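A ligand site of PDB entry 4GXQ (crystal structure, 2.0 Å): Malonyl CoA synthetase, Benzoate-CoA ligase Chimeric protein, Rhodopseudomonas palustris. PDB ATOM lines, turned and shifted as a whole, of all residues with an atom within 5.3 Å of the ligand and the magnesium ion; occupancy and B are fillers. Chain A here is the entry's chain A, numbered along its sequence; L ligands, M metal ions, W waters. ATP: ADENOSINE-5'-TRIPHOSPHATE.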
ATOM      1  N   THR A 163      19.791 -13.821  34.026  1.00  0.00           N
ATOM      2  CA  THR A 163      19.888 -13.936  32.578  1.00  0.00           C
ATOM      3  C   THR A 163      18.502 -13.769  31.930  1.00  0.00           C
ATOM      4  O   THR A 163      17.490 -13.839  32.624  1.00  0.00           O
ATOM      5  CB  THR A 163      20.462 -15.307  32.182  1.00  0.00           C
ATOM      6  OG1 THR A 163      19.665 -16.337  32.782  1.00  0.00           O
ATOM      7  CG2 THR A 163      21.884 -15.425  32.669  1.00  0.00           C
ATOM      8  N   SER A 164      18.462 -13.550  30.626  1.00  0.00           N
ATOM      9  CA  SER A 164      17.224 -13.130  29.966  1.00  0.00           C
ATOM     10  C   SER A 164      16.182 -14.237  29.823  1.00  0.00           C
ATOM     11  O   SER A 164      15.024 -13.967  29.503  1.00  0.00           O
ATOM     12  CB  SER A 164      17.534 -12.537  28.603  1.00  0.00           C
ATOM     13  OG  SER A 164      18.238 -11.316  28.755  1.00  0.00           O
ATOM     14  N   GLY A 165      16.581 -15.475  30.076  1.00  0.00           N
ATOM     15  CA  GLY A 165      15.653 -16.626  30.003  1.00  0.00           C
ATOM     16  C   GLY A 165      15.514 -17.225  28.616  1.00  0.00           C
ATOM     17  O   GLY A 165      14.582 -18.003  28.369  1.00  0.00           O
ATOM     18  N   THR A 166      16.435 -16.900  27.710  1.00  0.00           N
ATOM     19  CA  THR A 166      16.284 -17.305  26.293  1.00  0.00           C
ATOM     20  C   THR A 166      16.377 -18.824  26.072  1.00  0.00           C
ATOM     21  O   THR A 166      15.561 -19.398  25.327  1.00  0.00           O
ATOM     22  CB  THR A 166      17.269 -16.532  25.381  1.00  0.00           C
ATOM     23  OG1 THR A 166      17.044 -15.125  25.518  1.00  0.00           O
ATOM     24  CG2 THR A 166      17.072 -16.911  23.907  1.00  0.00           C
ATOM     25  N   THR A 167      17.339 -19.463  26.722  1.00  0.00           N
ATOM     26  CA  THR A 167      17.581 -20.894  26.549  1.00  0.00           C
ATOM     27  C   THR A 167      16.878 -21.762  27.594  1.00  0.00           C
ATOM     28  O   THR A 167      16.856 -22.976  27.495  1.00  0.00           O
ATOM     29  CB  THR A 167      19.097 -21.206  26.588  1.00  0.00           C
ATOM     30  OG1 THR A 167      19.611 -20.962  27.900  1.00  0.00           O
ATOM     31  CG2 THR A 167      19.856 -20.353  25.567  1.00  0.00           C
ATOM     32  N   GLY A 168      16.294 -21.126  28.590  1.00  0.00           N
ATOM     33  CA  GLY A 168      15.704 -21.833  29.715  1.00  0.00           C
ATOM     34  C   GLY A 168      15.433 -20.844  30.832  1.00  0.00           C
ATOM     35  O   GLY A 168      15.599 -19.646  30.661  1.00  0.00           O
ATOM     36  N   ARG A 169      14.991 -21.360  31.973  1.00  0.00           N
ATOM     37  CA  ARG A 169      14.664 -20.539  33.139  1.00  0.00           C
ATOM     38  C   ARG A 169      15.849 -19.662  33.530  1.00  0.00           C
ATOM     39  O   ARG A 169      16.973 -20.152  33.650  1.00  0.00           O
ATOM     40  CB  ARG A 169      14.280 -21.458  34.294  1.00  0.00           C
ATOM     41  CG  ARG A 169      14.259 -20.818  35.682  1.00  0.00           C
ATOM     42  CD  ARG A 169      13.503 -21.696  36.672  1.00  0.00           C
ATOM     43  NE  ARG A 169      12.112 -21.269  36.861  1.00  0.00           N
ATOM     44  CZ  ARG A 169      11.133 -22.031  37.376  1.00  0.00           C
ATOM     45  NH1 ARG A 169      11.374 -23.283  37.740  1.00  0.00           N
ATOM     46  NH2 ARG A 169       9.908 -21.534  37.513  1.00  0.00           N
ATOM     47  N   SER A 170      15.600 -18.376  33.728  1.00  0.00           N
ATOM     48  CA  SER A 170      16.670 -17.418  34.025  1.00  0.00           C
ATOM     49  C   SER A 170      17.485 -17.825  35.240  1.00  0.00           C
ATOM     50  O   SER A 170      16.933 -18.312  36.224  1.00  0.00           O
ATOM     51  CB  SER A 170      16.077 -16.039  34.273  1.00  0.00           C
ATOM     52  OG  SER A 170      15.351 -15.583  33.155  1.00  0.00           O
ATOM     53  N   MLY A 171      18.799 -17.598  35.165  1.00  0.00           N
ATOM     54  CA  MLY A 171      19.718 -17.890  36.284  1.00  0.00           C
ATOM     55  CB  MLY A 171      20.881 -18.737  35.773  1.00  0.00           C
ATOM     56  CG  MLY A 171      20.413 -19.997  35.032  1.00  0.00           C
ATOM     57  CD  MLY A 171      21.592 -20.893  34.634  1.00  0.00           C
ATOM     58  CE  MLY A 171      22.258 -20.475  33.324  1.00  0.00           C
ATOM     59  NZ  MLY A 171      21.373 -20.655  32.147  1.00  0.00           N
ATOM     60  CH1 MLY A 171      21.953 -19.953  30.991  1.00  0.00           C
ATOM     61  CH2 MLY A 171      21.204 -22.076  31.812  1.00  0.00           C
ATOM     62  C   MLY A 171      20.282 -16.604  36.844  1.00  0.00           C
ATOM     63  O   MLY A 171      20.503 -15.643  36.103  1.00  0.00           O
ATOM     64  N   HIS A 207      18.632  -4.972  32.628  1.00  0.00           N
ATOM     65  CA  HIS A 207      19.560  -5.768  31.821  1.00  0.00           C
ATOM     66  C   HIS A 207      20.941  -5.107  31.833  1.00  0.00           C
ATOM     67  O   HIS A 207      21.050  -3.886  31.973  1.00  0.00           O
ATOM     68  CB  HIS A 207      19.009  -5.891  30.400  1.00  0.00           C
ATOM     69  CG  HIS A 207      19.839  -6.749  29.507  1.00  0.00           C
ATOM     70  ND1 HIS A 207      20.924  -6.264  28.791  1.00  0.00           N
ATOM     71  CD2 HIS A 207      19.727  -8.059  29.160  1.00  0.00           C
ATOM     72  CE1 HIS A 207      21.458  -7.238  28.079  1.00  0.00           C
ATOM     73  NE2 HIS A 207      20.752  -8.337  28.282  1.00  0.00           N
ATOM     74  N   SER A 275      26.014  -1.045  18.874  1.00  0.00           N
ATOM     75  CA  SER A 275      25.007  -2.101  18.898  1.00  0.00           C
ATOM     76  C   SER A 275      25.460  -3.283  19.735  1.00  0.00           C
ATOM     77  O   SER A 275      26.627  -3.692  19.684  1.00  0.00           O
ATOM     78  CB  SER A 275      24.681  -2.607  17.484  1.00  0.00           C
ATOM     79  OG  SER A 275      23.677  -3.596  17.560  1.00  0.00           O
ATOM     80  N   GLY A 276      24.524  -3.845  20.486  1.00  0.00           N
ATOM     81  CA  GLY A 276      24.817  -4.954  21.365  1.00  0.00           C
ATOM     82  C   GLY A 276      23.597  -5.789  21.670  1.00  0.00           C
ATOM     83  O   GLY A 276      22.502  -5.436  21.270  1.00  0.00           O
ATOM     84  N   SER A 277      23.836  -6.931  22.337  1.00  0.00           N
ATOM     85  CA  SER A 277      22.818  -7.753  22.997  1.00  0.00           C
ATOM     86  C   SER A 277      22.144  -8.776  22.075  1.00  0.00           C
ATOM     87  O   SER A 277      21.457  -9.659  22.570  1.00  0.00           O
ATOM     88  CB  SER A 277      21.751  -6.909  23.687  1.00  0.00           C
ATOM     89  OG  SER A 277      22.321  -5.817  24.400  1.00  0.00           O
ATOM     90  N   ALA A 278      22.307  -8.626  20.768  1.00  0.00           N
ATOM     91  CA  ALA A 278      21.815  -9.593  19.788  1.00  0.00           C
ATOM     92  C   ALA A 278      22.615  -9.372  18.510  1.00  0.00           C
ATOM     93  O   ALA A 278      23.312  -8.339  18.377  1.00  0.00           O
ATOM     94  CB  ALA A 278      20.314  -9.426  19.538  1.00  0.00           C
ATOM     95  N   PRO A 279      22.564 -10.340  17.584  1.00  0.00           N
ATOM     96  CA  PRO A 279      23.412 -10.181  16.388  1.00  0.00           C
ATOM     97  C   PRO A 279      22.984  -8.993  15.543  1.00  0.00           C
ATOM     98  O   PRO A 279      21.830  -8.917  15.156  1.00  0.00           O
ATOM     99  CB  PRO A 279      23.184 -11.488  15.611  1.00  0.00           C
ATOM    100  CG  PRO A 279      22.596 -12.441  16.583  1.00  0.00           C
ATOM    101  CD  PRO A 279      21.862 -11.623  17.607  1.00  0.00           C
ATOM    102  N   LEU A 280      23.898  -8.059  15.289  1.00  0.00           N
ATOM    103  CA  LEU A 280      23.674  -7.056  14.274  1.00  0.00           C
ATOM    104  C   LEU A 280      24.026  -7.656  12.908  1.00  0.00           C
ATOM    105  O   LEU A 280      25.205  -7.920  12.637  1.00  0.00           O
ATOM    106  CB  LEU A 280      24.555  -5.829  14.536  1.00  0.00           C
ATOM    107  CG  LEU A 280      24.336  -4.664  13.570  1.00  0.00           C
ATOM    108  CD1 LEU A 280      22.960  -4.055  13.805  1.00  0.00           C
ATOM    109  CD2 LEU A 280      25.426  -3.614  13.729  1.00  0.00           C
ATOM    110  N   GLU A 298      29.878  -2.669  16.939  1.00  0.00           N
ATOM    111  CA  GLU A 298      29.189  -3.752  17.628  1.00  0.00           C
ATOM    112  C   GLU A 298      30.099  -4.385  18.660  1.00  0.00           C
ATOM    113  O   GLU A 298      31.300  -4.595  18.423  1.00  0.00           O
ATOM    114  CB  GLU A 298      28.720  -4.832  16.647  1.00  0.00           C
ATOM    115  CG  GLU A 298      28.031  -6.017  17.294  1.00  0.00           C
ATOM    116  CD  GLU A 298      27.449  -7.012  16.300  1.00  0.00           C
ATOM    117  OE1 GLU A 298      27.892  -7.028  15.124  1.00  0.00           O
ATOM    118  OE2 GLU A 298      26.546  -7.768  16.700  1.00  0.00           O
ATOM    119  N   ARG A 299      29.516  -4.680  19.814  1.00  0.00           N
ATOM    120  CA  ARG A 299      30.201  -5.398  20.870  1.00  0.00           C
ATOM    121  C   ARG A 299      29.363  -6.563  21.373  1.00  0.00           C
ATOM    122  O   ARG A 299      28.139  -6.615  21.183  1.00  0.00           O
ATOM    123  CB  ARG A 299      30.609  -4.441  22.006  1.00  0.00           C
ATOM    124  CG  ARG A 299      29.634  -4.277  23.157  1.00  0.00           C
ATOM    125  CD  ARG A 299      28.341  -3.610  22.718  1.00  0.00           C
ATOM    126  NE  ARG A 299      27.412  -3.453  23.841  1.00  0.00           N
ATOM    127  CZ  ARG A 299      26.733  -4.440  24.390  1.00  0.00           C
ATOM    128  NH1 ARG A 299      25.918  -4.201  25.401  1.00  0.00           N
ATOM    129  NH2 ARG A 299      26.871  -5.685  23.942  1.00  0.00           N
ATOM    130  N   TYR A 300      30.040  -7.507  22.023  1.00  0.00           N
ATOM    131  CA  TYR A 300      29.431  -8.744  22.484  1.00  0.00           C
ATOM    132  C   TYR A 300      29.683  -8.943  23.943  1.00  0.00           C
ATOM    133  O   TYR A 300      30.826  -8.862  24.397  1.00  0.00           O
ATOM    134  CB  TYR A 300      30.011  -9.921  21.691  1.00  0.00           C
ATOM    135  CG  TYR A 300      29.959 -11.288  22.367  1.00  0.00           C
ATOM    136  CD1 TYR A 300      28.746 -11.894  22.700  1.00  0.00           C
ATOM    137  CD2 TYR A 300      31.133 -12.021  22.555  1.00  0.00           C
ATOM    138  CE1 TYR A 300      28.709 -13.173  23.266  1.00  0.00           C
ATOM    139  CE2 TYR A 300      31.115 -13.284  23.119  1.00  0.00           C
ATOM    140  CZ  TYR A 300      29.914 -13.865  23.458  1.00  0.00           C
ATOM    141  OH  TYR A 300      29.930 -15.127  24.015  1.00  0.00           O
ATOM    142  N   GLY A 301      28.613  -9.238  24.663  1.00  0.00           N
ATOM    143  CA  GLY A 301      28.687  -9.514  26.084  1.00  0.00           C
ATOM    144  C   GLY A 301      27.582 -10.439  26.525  1.00  0.00           C
ATOM    145  O   GLY A 301      26.741 -10.859  25.707  1.00  0.00           O
ATOM    146  N   MET A 302      27.611 -10.776  27.813  1.00  0.00           N
ATOM    147  CA  MET A 302      26.623 -11.638  28.445  1.00  0.00           C
ATOM    148  C   MET A 302      26.371 -11.127  29.828  1.00  0.00           C
ATOM    149  O   MET A 302      27.223 -10.457  30.417  1.00  0.00           O
ATOM    150  CB  MET A 302      27.149 -13.084  28.582  1.00  0.00           C
ATOM    151  CG  MET A 302      27.680 -13.725  27.320  1.00  0.00           C
ATOM    152  SD  MET A 302      28.464 -15.323  27.645  1.00  0.00           S
ATOM    153  CE  MET A 302      27.172 -16.142  28.583  1.00  0.00           C
ATOM    154  N   THR A 303      25.202 -11.467  30.377  1.00  0.00           N
ATOM    155  CA  THR A 303      24.914 -11.205  31.774  1.00  0.00           C
ATOM    156  C   THR A 303      26.066 -11.683  32.671  1.00  0.00           C
ATOM    157  O   THR A 303      26.498 -10.974  33.579  1.00  0.00           O
ATOM    158  CB  THR A 303      23.576 -11.836  32.196  1.00  0.00           C
ATOM    159  OG1 THR A 303      22.513 -11.224  31.449  1.00  0.00           O
ATOM    160  CG2 THR A 303      23.313 -11.636  33.677  1.00  0.00           C
ATOM    161  N   GLU A 304      26.581 -12.891  32.385  1.00  0.00           N
ATOM    162  CA  GLU A 304      27.607 -13.533  33.207  1.00  0.00           C
ATOM    163  C   GLU A 304      28.993 -12.943  33.096  1.00  0.00           C
ATOM    164  O   GLU A 304      29.821 -13.172  33.972  1.00  0.00           O
ATOM    165  CB  GLU A 304      27.695 -15.025  32.872  1.00  0.00           C
ATOM    166  CG  GLU A 304      26.438 -15.811  33.211  1.00  0.00           C
ATOM    167  CD  GLU A 304      25.512 -15.968  32.015  1.00  0.00           C
ATOM    168  OE1 GLU A 304      25.424 -15.043  31.185  1.00  0.00           O
ATOM    169  OE2 GLU A 304      24.902 -17.053  31.913  1.00  0.00           O
ATOM    170  N   VAL A 322      32.032  -9.314  16.022  1.00  0.00           N
ATOM    171  CA  VAL A 322      31.840  -8.624  17.286  1.00  0.00           C
ATOM    172  C   VAL A 322      33.169  -8.126  17.879  1.00  0.00           C
ATOM    173  O   VAL A 322      33.227  -7.712  19.038  1.00  0.00           O
ATOM    174  CB  VAL A 322      31.080  -9.500  18.312  1.00  0.00           C
ATOM    175  CG1 VAL A 322      29.642  -9.727  17.839  1.00  0.00           C
ATOM    176  CG2 VAL A 322      31.790 -10.821  18.538  1.00  0.00           C
ATOM    177  N   THR A 380      30.893 -19.950  27.265  1.00  0.00           N
ATOM    178  CA  THR A 380      29.830 -18.981  26.961  1.00  0.00           C
ATOM    179  C   THR A 380      28.506 -19.622  26.548  1.00  0.00           C
ATOM    180  O   THR A 380      27.447 -19.117  26.880  1.00  0.00           O
ATOM    181  CB  THR A 380      30.223 -17.983  25.861  1.00  0.00           C
ATOM    182  OG1 THR A 380      30.464 -18.678  24.627  1.00  0.00           O
ATOM    183  CG2 THR A 380      31.460 -17.194  26.288  1.00  0.00           C
ATOM    184  N   ASP A 382      28.065 -19.968  23.372  1.00  0.00           N
ATOM    185  CA  ASP A 382      27.977 -19.373  22.045  1.00  0.00           C
ATOM    186  C   ASP A 382      29.026 -20.002  21.130  1.00  0.00           C
ATOM    187  O   ASP A 382      30.205 -20.106  21.482  1.00  0.00           O
ATOM    188  CB  ASP A 382      28.206 -17.856  22.136  1.00  0.00           C
ATOM    189  CG  ASP A 382      27.079 -17.120  22.873  1.00  0.00           C
ATOM    190  OD1 ASP A 382      25.904 -17.454  22.630  1.00  0.00           O
ATOM    191  OD2 ASP A 382      27.377 -16.209  23.683  1.00  0.00           O
ATOM    192  N   ILE A 394      30.370 -14.634  15.916  1.00  0.00           N
ATOM    193  CA  ILE A 394      29.435 -15.512  16.586  1.00  0.00           C
ATOM    194  C   ILE A 394      28.521 -16.163  15.558  1.00  0.00           C
ATOM    195  O   ILE A 394      27.794 -15.485  14.815  1.00  0.00           O
ATOM    196  CB  ILE A 394      28.631 -14.780  17.643  1.00  0.00           C
ATOM    197  CG1 ILE A 394      29.579 -14.288  18.746  1.00  0.00           C
ATOM    198  CG2 ILE A 394      27.569 -15.692  18.225  1.00  0.00           C
ATOM    199  CD1 ILE A 394      28.896 -13.375  19.734  1.00  0.00           C
ATOM    200  N   ARG A 397      24.030 -19.612  19.074  1.00  0.00           N
ATOM    201  CA  ARG A 397      24.040 -20.254  20.387  1.00  0.00           C
ATOM    202  C   ARG A 397      24.170 -21.758  20.197  1.00  0.00           C
ATOM    203  O   ARG A 397      23.595 -22.313  19.250  1.00  0.00           O
ATOM    204  CB  ARG A 397      22.738 -20.005  21.139  1.00  0.00           C
ATOM    205  CG  ARG A 397      22.377 -18.558  21.421  1.00  0.00           C
ATOM    206  CD  ARG A 397      21.009 -18.499  22.057  1.00  0.00           C
ATOM    207  NE  ARG A 397      20.561 -17.123  22.305  1.00  0.00           N
ATOM    208  CZ  ARG A 397      20.757 -16.439  23.430  1.00  0.00           C
ATOM    209  NH1 ARG A 397      20.301 -15.193  23.523  1.00  0.00           N
ATOM    210  NH2 ARG A 397      21.371 -16.986  24.471  1.00  0.00           N
ATOM    211  N   ASN A 487      11.921 -11.064  23.085  1.00  0.00           N
ATOM    212  CA  ASN A 487      11.809 -10.700  24.479  1.00  0.00           C
ATOM    213  C   ASN A 487      11.796  -9.187  24.593  1.00  0.00           C
ATOM    214  O   ASN A 487      11.875  -8.482  23.575  1.00  0.00           O
ATOM    215  CB  ASN A 487      12.917 -11.352  25.318  1.00  0.00           C
ATOM    216  CG  ASN A 487      14.311 -10.794  25.044  1.00  0.00           C
ATOM    217  OD1 ASN A 487      14.485  -9.813  24.311  1.00  0.00           O
ATOM    218  ND2 ASN A 487      15.311 -11.421  25.631  1.00  0.00           N
HETATM  219  PG  ATP L   1      19.757 -17.158  29.047  1.00  0.00           P
HETATM  220  O1G ATP L   1      18.852 -17.161  30.236  1.00  0.00           O
HETATM  221  O2G ATP L   1      21.214 -17.093  29.454  1.00  0.00           O
HETATM  222  O3G ATP L   1      19.454 -18.234  28.021  1.00  0.00           O
HETATM  223  PB  ATP L   1      20.373 -14.926  27.341  1.00  0.00           P
HETATM  224  O1B ATP L   1      19.653 -14.285  26.195  1.00  0.00           O
HETATM  225  O2B ATP L   1      21.626 -15.725  26.999  1.00  0.00           O
HETATM  226  O3B ATP L   1      19.371 -15.802  28.252  1.00  0.00           O
HETATM  227  PA  ATP L   1      21.686 -12.473  28.020  1.00  0.00           P
HETATM  228  O1A ATP L   1      22.807 -12.459  29.021  1.00  0.00           O
HETATM  229  O2A ATP L   1      20.796 -11.258  27.897  1.00  0.00           O
HETATM  230  O3A ATP L   1      20.809 -13.776  28.404  1.00  0.00           O
HETATM  231  O5' ATP L   1      22.243 -12.602  26.534  1.00  0.00           O
HETATM  232  C5' ATP L   1      23.612 -12.938  26.264  1.00  0.00           C
HETATM  233  C4' ATP L   1      23.667 -13.629  24.928  1.00  0.00           C
HETATM  234  O4' ATP L   1      23.235 -12.761  23.883  1.00  0.00           O
HETATM  235  C3' ATP L   1      25.075 -14.041  24.520  1.00  0.00           C
HETATM  236  O3' ATP L   1      25.502 -15.214  25.185  1.00  0.00           O
HETATM  237  C2' ATP L   1      24.886 -14.222  23.035  1.00  0.00           C
HETATM  238  O2' ATP L   1      24.251 -15.484  22.812  1.00  0.00           O
HETATM  239  C1' ATP L   1      23.931 -13.094  22.678  1.00  0.00           C
HETATM  240  N9  ATP L   1      24.617 -11.869  22.187  1.00  0.00           N
HETATM  241  C8  ATP L   1      24.901 -10.760  22.916  1.00  0.00           C
HETATM  242  N7  ATP L   1      25.525  -9.831  22.159  1.00  0.00           N
HETATM  243  C5  ATP L   1      25.628 -10.351  20.919  1.00  0.00           C
HETATM  244  C6  ATP L   1      26.175  -9.920  19.622  1.00  0.00           C
HETATM  245  N6  ATP L   1      26.745  -8.696  19.456  1.00  0.00           N
HETATM  246  N1  ATP L   1      26.090 -10.785  18.585  1.00  0.00           N
HETATM  247  C2  ATP L   1      25.521 -11.998  18.694  1.00  0.00           C
HETATM  248  N3  ATP L   1      25.006 -12.457  19.834  1.00  0.00           N
HETATM  249  C4  ATP L   1      25.023 -11.682  20.955  1.00  0.00           C
HETATM  250 MG    MG M   1      22.690 -16.886  28.197  1.00  0.00          MG
HETATM  251  O   HOH W   1      24.205 -16.894  26.637  1.00  0.00           O
HETATM  252  O   HOH W   2      21.306 -10.026  25.235  1.00  0.00           O
HETATM  253  O   HOH W   3      23.852 -15.167  19.746  1.00  0.00           O
HETATM  254  O   HOH W   4      23.988 -17.976  29.341  1.00  0.00           O
HETATM  255  O   HOH W   5      19.018 -11.886  24.850  1.00  0.00           O
HETATM  256  O   HOH W   6      21.930 -18.775  27.248  1.00  0.00           O
HETATM  257  O   HOH W   7      26.965 -11.104  15.964  1.00  0.00           O
HETATM  258  O   HOH W   8      20.493 -12.364  22.274  1.00  0.00           O
HETATM  259  O   HOH W   9      23.641 -15.146  29.101  1.00  0.00           O
HETATM  260  O   HOH W  10      18.785 -19.860  31.606  1.00  0.00           O
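The magnesium ion is bound by an oxygen (O2G) of the ligand (1.9 Å), an oxygen (O2B) of the ligand (2.0 Å), water W4 (2.0 Å), water W1 (2.2 Å), water W9 (2.2 Å) and water W6 (2.2 Å). The magnesium ion has six donor atoms within binding distance.
Water W9 bridges OE1 of Glu 304 and O1A of the ligand. Water W6 lies within hydrogen-bond range of an oxygen (O3G) of the ligand, the side-chain hydroxyl (OG1) of Thr 167 and the guanidinium group (NH2) of Arg 397. Water W7 lies within hydrogen-bond range of N1 of the ligand (2.8 Å) and OE2 of Glu 298 (3.4 Å). Water W2 lies within hydrogen-bond range of O of Ser 277 and O2A of the ligand. Water W10 lies within hydrogen-bond range of the backbone carbonyl oxygen (O) of Arg 169 (2.7 Å), an oxygen (O1G) of the ligand (3.0 Å) and the backbone carbonyl oxygen (O) of Gly 168 (3.3 Å). Water W8 lies within hydrogen-bond range of O of Ser 277, NH1 of Arg 397 and O4' of the ligand.
The backbone NH (N) of Gly 165 sits at hydrogen-bond distance from the side-chain hydroxyl (OG) of Ser 170 (3.3 Å). OD2 of Asp 382 is in hydrogen-bond range of OH of Tyr 300, 2.8 Å away. The backbone NH (N) of Arg 299 sits at hydrogen-bond distance from the backbone carbonyl oxygen (O) of Ser 275 (3.1 Å). The side-chain hydroxyl of Thr 163 sits at hydrogen-bond distance from N of MLY 171, at 2.8 Å. The backbone NH of Leu 280 sits at hydrogen-bond distance from the side-chain carboxylate of Glu 298. The backbone carbonyl oxygen (O) of Thr 163 lies within hydrogen-bond range of the side-chain hydroxyl (OG) of Ser 170 (2.8 Å). N of Asp 382 sits at hydrogen-bond distance from OG1 of Thr 380.
N of Thr 167 lies within hydrogen-bond range of O3G of the ligand. O1A of the ligand is in hydrogen-bond range of N of Thr 303. O3B of the ligand is in hydrogen-bond range of N of Thr 166, at 3.2 Å. NE2 of His 207 is in hydrogen-bond range of O2A of the ligand. O of Arg 299 lies within hydrogen-bond range of N6 of the ligand, 3.0 Å away. O1B of the ligand is in hydrogen-bond range of OG1 of Thr 166. The backbone NH of Ser 164 is in hydrogen-bond range of an oxygen (O3A) of the ligand, 3.2 Å away. The backbone NH of Ser 277 is in hydrogen-bond range of a nitrogen (N7) of the ligand. The side-chain hydroxyl (OG1) of Thr 303 is in hydrogen-bond range of an oxygen (O1A) of the ligand, at 2.7 Å. The guanidinium group of Arg 397 lies within salt-bridge range of an oxygen (O1B) of the ligand (2.9 Å). An oxygen (O1G) of the ligand lies within hydrogen-bond range of the backbone NH (N) of Gly 165, at 2.8 Å. O2A of the ligand lies within hydrogen-bond range of OG of Ser 164 (2.7 Å). The side-chain hydroxyl (OG1) of Thr 163 lies within hydrogen-bond range of an oxygen (O1G) of the ligand, at 2.8 Å. OE2 of Glu 298 is in hydrogen-bond range of N6 of the ligand (2.9 Å). An oxygen (O2') of the ligand is in hydrogen-bond range of the side-chain carboxylate of Asp 382 (2.6 Å). OG1 of Thr 167 lies within hydrogen-bond range of O3G of the ligand (2.7 Å).
Residues that only touch the magnesium ion: Arg 397 (3.95 Å). Of the 29 residues printed, 1 comes within 4 Å of the magnesium ion.
MLY 171 touches the ligand (CH1 to O2G, 3.3 Å). O of Ala 278 touches C6 of the ligand, 3.5 Å away. Pro 279 touches the ligand. Tyr 300 touches the ligand (CD1 to N7, 3.9 Å). Gly 301 touches the ligand. CG of Met 302 touches O3' of the ligand, 3.4 Å away. Val 322 touches the ligand. Ile 394 touches the ligand. Of the 29 residues printed, 20 come within 4 Å of the ligand. The nearest printed residue that does not touch the ligand is Gly 168 (4.1 Å).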
